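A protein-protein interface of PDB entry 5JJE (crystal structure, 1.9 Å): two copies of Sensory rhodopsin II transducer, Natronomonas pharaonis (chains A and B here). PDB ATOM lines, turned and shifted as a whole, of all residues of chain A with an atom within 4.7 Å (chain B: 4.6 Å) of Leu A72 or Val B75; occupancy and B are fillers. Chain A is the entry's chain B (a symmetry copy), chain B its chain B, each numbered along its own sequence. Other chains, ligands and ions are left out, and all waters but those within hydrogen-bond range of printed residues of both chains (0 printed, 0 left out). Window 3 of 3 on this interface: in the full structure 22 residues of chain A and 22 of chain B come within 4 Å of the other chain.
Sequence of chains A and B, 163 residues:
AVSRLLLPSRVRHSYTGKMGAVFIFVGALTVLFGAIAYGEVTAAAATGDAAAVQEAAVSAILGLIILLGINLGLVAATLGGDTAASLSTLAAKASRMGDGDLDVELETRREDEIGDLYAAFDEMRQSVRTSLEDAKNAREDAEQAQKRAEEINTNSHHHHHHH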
ATOM      1  N   LEU A  68      -1.398  33.099  -1.248  1.00  0.00           N
ATOM      2  CA  LEU A  68      -2.198  31.988  -1.776  1.00  0.00           C
ATOM      3  C   LEU A  68      -3.600  32.026  -1.204  1.00  0.00           C
ATOM      4  O   LEU A  68      -4.587  31.893  -1.933  1.00  0.00           O
ATOM      5  CB  LEU A  68      -1.590  30.613  -1.453  1.00  0.00           C
ATOM      6  CG  LEU A  68      -2.697  29.537  -1.551  1.00  0.00           C
ATOM      7  CD1 LEU A  68      -2.967  29.084  -2.994  1.00  0.00           C
ATOM      8  CD2 LEU A  68      -2.507  28.338  -0.636  1.00  0.00           C
ATOM      9  N   GLY A  69      -3.688  32.209   0.111  1.00  0.00           N
ATOM     10  CA  GLY A  69      -4.979  32.298   0.769  1.00  0.00           C
ATOM     11  C   GLY A  69      -5.838  33.399   0.177  1.00  0.00           C
ATOM     12  O   GLY A  69      -7.033  33.213  -0.066  1.00  0.00           O
ATOM     13  N   ILE A  70      -5.231  34.558  -0.067  1.00  0.00           N
ATOM     14  CA  ILE A  70      -5.971  35.664  -0.656  1.00  0.00           C
ATOM     15  C   ILE A  70      -6.437  35.320  -2.074  1.00  0.00           C
ATOM     16  O   ILE A  70      -7.606  35.530  -2.425  1.00  0.00           O
ATOM     17  CB  ILE A  70      -5.119  36.943  -0.712  1.00  0.00           C
ATOM     18  CG1 ILE A  70      -4.740  37.388   0.708  1.00  0.00           C
ATOM     19  CG2 ILE A  70      -5.871  38.047  -1.452  1.00  0.00           C
ATOM     20  CD1 ILE A  70      -3.682  38.503   0.761  1.00  0.00           C
ATOM     21  N   ASN A  71      -5.520  34.828  -2.899  1.00  0.00           N
ATOM     22  CA  ASN A  71      -5.865  34.518  -4.279  1.00  0.00           C
ATOM     23  C   ASN A  71      -6.935  33.422  -4.347  1.00  0.00           C
ATOM     24  O   ASN A  71      -7.895  33.526  -5.112  1.00  0.00           O
ATOM     25  CB  ASN A  71      -4.636  34.067  -5.058  1.00  0.00           C
ATOM     26  CG  ASN A  71      -3.578  35.146  -5.182  1.00  0.00           C
ATOM     27  OD1 ASN A  71      -3.867  36.330  -5.117  1.00  0.00           O
ATOM     28  ND2 ASN A  71      -2.340  34.725  -5.393  1.00  0.00           N
ATOM     29  N   LEU A  72      -6.751  32.375  -3.547  1.00  0.00           N
ATOM     30  CA  LEU A  72      -7.691  31.258  -3.484  1.00  0.00           C
ATOM     31  C   LEU A  72      -9.039  31.722  -2.994  1.00  0.00           C
ATOM     32  O   LEU A  72     -10.079  31.290  -3.497  1.00  0.00           O
ATOM     33  CB  LEU A  72      -7.185  30.186  -2.530  1.00  0.00           C
ATOM     34  CG  LEU A  72      -6.529  28.970  -3.148  1.00  0.00           C
ATOM     35  CD1 LEU A  72      -6.431  27.908  -2.084  1.00  0.00           C
ATOM     36  CD2 LEU A  72      -7.339  28.490  -4.329  1.00  0.00           C
ATOM     37  N   GLY A  73      -9.009  32.593  -1.993  1.00  0.00           N
ATOM     38  CA  GLY A  73     -10.211  33.208  -1.468  1.00  0.00           C
ATOM     39  C   GLY A  73     -10.930  33.997  -2.533  1.00  0.00           C
ATOM     40  O   GLY A  73     -12.141  33.855  -2.690  1.00  0.00           O
ATOM     41  N   LEU A  74     -10.194  34.830  -3.268  1.00  0.00           N
ATOM     42  CA  LEU A  74     -10.771  35.612  -4.356  1.00  0.00           C
ATOM     43  C   LEU A  74     -11.388  34.723  -5.446  1.00  0.00           C
ATOM     44  O   LEU A  74     -12.501  34.967  -5.918  1.00  0.00           O
ATOM     45  CB  LEU A  74      -9.698  36.510  -4.975  1.00  0.00           C
ATOM     46  CG  LEU A  74     -10.002  37.294  -6.256  1.00  0.00           C
ATOM     47  CD1 LEU A  74     -11.243  38.169  -6.114  1.00  0.00           C
ATOM     48  CD2 LEU A  74      -8.797  38.159  -6.635  1.00  0.00           C
ATOM     49  N   VAL A  75     -10.641  33.703  -5.850  1.00  0.00           N
ATOM     50  CA  VAL A  75     -11.070  32.779  -6.897  1.00  0.00           C
ATOM     51  C   VAL A  75     -12.298  31.970  -6.482  1.00  0.00           C
ATOM     52  O   VAL A  75     -13.303  31.936  -7.198  1.00  0.00           O
ATOM     53  CB  VAL A  75      -9.906  31.835  -7.295  1.00  0.00           C
ATOM     54  CG1 VAL A  75     -10.418  30.640  -8.084  1.00  0.00           C
ATOM     55  CG2 VAL A  75      -8.851  32.620  -8.084  1.00  0.00           C
ATOM     56  N   ALA A  76     -12.212  31.319  -5.328  1.00  0.00           N
ATOM     57  CA  ALA A  76     -13.329  30.545  -4.804  1.00  0.00           C
ATOM     58  C   ALA A  76     -14.565  31.424  -4.709  1.00  0.00           C
ATOM     59  O   ALA A  76     -15.663  31.017  -5.092  1.00  0.00           O
ATOM     60  CB  ALA A  76     -12.986  29.958  -3.440  1.00  0.00           C
ATOM     61  N   ALA A  77     -14.377  32.640  -4.220  1.00  0.00           N
ATOM     62  CA  ALA A  77     -15.494  33.574  -4.059  1.00  0.00           C
ATOM     63  C   ALA A  77     -16.127  34.066  -5.362  1.00  0.00           C
ATOM     64  O   ALA A  77     -17.331  34.330  -5.399  1.00  0.00           O
ATOM     65  CB  ALA A  77     -15.082  34.753  -3.186  1.00  0.00           C
ATOM     66  N   MET B  19     -15.840  20.591  -2.809  1.00  0.00           N
ATOM     67  CA  MET B  19     -14.814  21.602  -2.823  1.00  0.00           C
ATOM     68  C   MET B  19     -14.038  21.664  -1.513  1.00  0.00           C
ATOM     69  O   MET B  19     -12.859  22.010  -1.484  1.00  0.00           O
ATOM     70  CB  MET B  19     -15.413  22.948  -3.194  1.00  0.00           C
ATOM     71  CG  MET B  19     -15.778  23.042  -4.654  1.00  0.00           C
ATOM     72  SD  MET B  19     -14.402  22.685  -5.762  1.00  0.00           S
ATOM     73  CE  MET B  19     -13.286  24.013  -5.361  1.00  0.00           C
ATOM     74  N   PHE B  23     -10.058  22.089  -0.854  1.00  0.00           N
ATOM     75  CA  PHE B  23      -9.449  23.284  -0.248  1.00  0.00           C
ATOM     76  C   PHE B  23      -8.510  22.956   0.911  1.00  0.00           C
ATOM     77  O   PHE B  23      -7.402  23.439   0.965  1.00  0.00           O
ATOM     78  CB  PHE B  23     -10.494  24.311   0.220  1.00  0.00           C
ATOM     79  CG  PHE B  23     -11.030  25.186  -0.868  1.00  0.00           C
ATOM     80  CD1 PHE B  23     -12.359  25.159  -1.206  1.00  0.00           C
ATOM     81  CD2 PHE B  23     -10.224  26.037  -1.545  1.00  0.00           C
ATOM     82  CE1 PHE B  23     -12.833  25.959  -2.187  1.00  0.00           C
ATOM     83  CE2 PHE B  23     -10.721  26.818  -2.543  1.00  0.00           C
ATOM     84  CZ  PHE B  23     -12.012  26.781  -2.851  1.00  0.00           C
ATOM     85  N   VAL B  26      -5.444  21.717  -0.270  1.00  0.00           N
ATOM     86  CA  VAL B  26      -4.644  22.788  -0.855  1.00  0.00           C
ATOM     87  C   VAL B  26      -3.997  23.629   0.239  1.00  0.00           C
ATOM     88  O   VAL B  26      -2.819  23.884   0.225  1.00  0.00           O
ATOM     89  CB  VAL B  26      -5.478  23.639  -1.834  1.00  0.00           C
ATOM     90  CG1 VAL B  26      -4.874  24.914  -2.063  1.00  0.00           C
ATOM     91  CG2 VAL B  26      -5.574  22.972  -3.123  1.00  0.00           C
ATOM     92  N   ASN B  71      -2.093  25.057  -7.292  1.00  0.00           N
ATOM     93  CA  ASN B  71      -3.314  25.082  -6.500  1.00  0.00           C
ATOM     94  C   ASN B  71      -4.450  25.776  -7.260  1.00  0.00           C
ATOM     95  O   ASN B  71      -5.583  25.291  -7.281  1.00  0.00           O
ATOM     96  CB  ASN B  71      -3.087  25.798  -5.175  1.00  0.00           C
ATOM     97  CG  ASN B  71      -2.088  25.093  -4.278  1.00  0.00           C
ATOM     98  OD1 ASN B  71      -1.883  23.894  -4.375  1.00  0.00           O
ATOM     99  ND2 ASN B  71      -1.482  25.849  -3.375  1.00  0.00           N
ATOM    100  N   LEU B  72      -4.133  26.914  -7.873  1.00  0.00           N
ATOM    101  CA  LEU B  72      -5.101  27.685  -8.651  1.00  0.00           C
ATOM    102  C   LEU B  72      -5.592  26.886  -9.832  1.00  0.00           C
ATOM    103  O   LEU B  72      -6.779  26.913 -10.165  1.00  0.00           O
ATOM    104  CB  LEU B  72      -4.467  28.964  -9.178  1.00  0.00           C
ATOM    105  CG  LEU B  72      -4.778  30.243  -8.430  1.00  0.00           C
ATOM    106  CD1 LEU B  72      -4.357  31.398  -9.299  1.00  0.00           C
ATOM    107  CD2 LEU B  72      -6.251  30.307  -8.107  1.00  0.00           C
ATOM    108  N   GLY B  73      -4.661  26.190 -10.472  1.00  0.00           N
ATOM    109  CA  GLY B  73      -4.980  25.297 -11.568  1.00  0.00           C
ATOM    110  C   GLY B  73      -5.922  24.207 -11.126  1.00  0.00           C
ATOM    111  O   GLY B  73      -6.918  23.947 -11.799  1.00  0.00           O
ATOM    112  N   LEU B  74      -5.616  23.564 -10.001  1.00  0.00           N
ATOM    113  CA  LEU B  74      -6.475  22.520  -9.452  1.00  0.00           C
ATOM    114  C   LEU B  74      -7.882  23.040  -9.122  1.00  0.00           C
ATOM    115  O   LEU B  74      -8.892  22.410  -9.446  1.00  0.00           O
ATOM    116  CB  LEU B  74      -5.838  21.933  -8.191  1.00  0.00           C
ATOM    117  CG  LEU B  74      -6.628  20.950  -7.321  1.00  0.00           C
ATOM    118  CD1 LEU B  74      -7.139  19.756  -8.120  1.00  0.00           C
ATOM    119  CD2 LEU B  74      -5.755  20.463  -6.162  1.00  0.00           C
ATOM    120  N   VAL B  75      -7.931  24.188  -8.456  1.00  0.00           N
ATOM    121  CA  VAL B  75      -9.189  24.804  -8.042  1.00  0.00           C
ATOM    122  C   VAL B  75     -10.038  25.235  -9.237  1.00  0.00           C
ATOM    123  O   VAL B  75     -11.213  24.873  -9.339  1.00  0.00           O
ATOM    124  CB  VAL B  75      -8.917  26.010  -7.105  1.00  0.00           C
ATOM    125  CG1 VAL B  75     -10.153  26.887  -6.972  1.00  0.00           C
ATOM    126  CG2 VAL B  75      -8.437  25.504  -5.739  1.00  0.00           C
ATOM    127  N   ALA B  76      -9.441  26.011 -10.135  1.00  0.00           N
ATOM    128  CA  ALA B  76     -10.133  26.456 -11.337  1.00  0.00           C
ATOM    129  C   ALA B  76     -10.669  25.254 -12.098  1.00  0.00           C
ATOM    130  O   ALA B  76     -11.812  25.254 -12.556  1.00  0.00           O
ATOM    131  CB  ALA B  76      -9.201  27.275 -12.222  1.00  0.00           C
ATOM    132  N   ALA B  77      -9.847  24.222 -12.207  1.00  0.00           N
ATOM    133  CA  ALA B  77     -10.240  23.014 -12.936  1.00  0.00           C
ATOM    134  C   ALA B  77     -11.366  22.201 -12.293  1.00  0.00           C
ATOM    135  O   ALA B  77     -12.155  21.574 -13.004  1.00  0.00           O
ATOM    136  CB  ALA B  77      -9.026  22.130 -13.198  1.00  0.00           C
ATOM    137  N   THR B  78     -11.447  22.190 -10.964  1.00  0.00           N
ATOM    138  CA  THR B  78     -12.490  21.400 -10.293  1.00  0.00           C
ATOM    139  C   THR B  78     -13.744  22.223  -9.972  1.00  0.00           C
ATOM    140  O   THR B  78     -14.866  21.716 -10.036  1.00  0.00           O
ATOM    141  CB  THR B  78     -11.982  20.757  -8.991  1.00  0.00           C
ATOM    142  OG1 THR B  78     -11.487  21.776  -8.113  1.00  0.00           O
ATOM    143  CG2 THR B  78     -10.865  19.764  -9.285  1.00  0.00           C
ATOM    144  N   LEU B  79     -13.611  23.494  -9.586  1.00  0.00           N
ATOM    145  CA  LEU B  79     -14.815  24.244  -9.306  1.00  0.00           C
ATOM    146  C   LEU B  79     -15.300  25.062 -10.472  1.00  0.00           C
ATOM    147  O   LEU B  79     -16.377  25.607 -10.388  1.00  0.00           O
ATOM    148  CB  LEU B  79     -14.793  25.039  -8.004  1.00  0.00           C
ATOM    149  CG  LEU B  79     -13.838  26.167  -7.645  1.00  0.00           C
ATOM    150  CD1 LEU B  79     -13.593  26.959  -8.828  1.00  0.00           C
ATOM    151  CD2 LEU B  79     -14.450  27.029  -6.628  1.00  0.00           C
ATOM    152  N   GLY B  80     -14.528  25.126 -11.551  1.00  0.00           N
ATOM    153  CA  GLY B  80     -15.048  25.615 -12.817  1.00  0.00           C
ATOM    154  C   GLY B  80     -15.961  24.605 -13.494  1.00  0.00           C
ATOM    155  O   GLY B  80     -16.309  23.579 -12.907  1.00  0.00           O
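The side-chain hydroxyl (OG1) of Thr B78 is in hydrogen-bond range of the backbone carbonyl oxygen (O) of Val B75.
Among the printed residues, merely in contact across the chains: Leu A72 with Val B26 (3.4 Å), Ala A76 with Phe B23 (3.4 Å), Leu A72 with Val B75 (3.5 Å), Val A75 with Leu B72 (3.5 Å), Leu A68 with Asn B71 (3.6 Å) and Val A75 with Val B75 (3.9 Å).
Of chain B, only Val B26 (3.4 Å) and Val B75 (3.5 Å) come within 4 Å of Leu A72.
Of the printed residues of chain A, Val B26 touches Leu A72.
Of the printed residues of chain A, Leu B72 touches Val A75 (3.5 Å).
Gly B73 touches none of the printed residues of chain A.
Leu B79 touches none of the printed residues of chain A.
The nearest printed residue of chain A that does not touch Val B75 is Ala A76 (5.2 Å).
The nearest printed residue of chain A that does not touch Val B26 is Leu A68 (4.4 Å).
Of the 10 printed residues of chain A, 4 touch a printed residue of chain B.
Printed residues of chain A that touch a printed residue of chain B: Leu A68, Leu A72, Val A75 and Ala A76.
Hydrophobic or aromatic side chains of chain A within 4 Å of the printed part of chain B: Leu A68, Leu A72, Val A75 and Ala A76.
Hydrophobic or aromatic side chains of chain B within 4 Å of the printed part of chain A: Phe B23, Val B26, Leu B72 and Val B75.
Among the printed residues, no Asp or Glu carboxylate lies within 4 Å of a Lys or Arg side-chain nitrogen of the other chain.
Leu A72 touches Val B75, and with the chains exchanged Val A75 touches Leu B72.
Val B75 touches its own counterpart, Val A75.
7 positions are printed for both chains.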
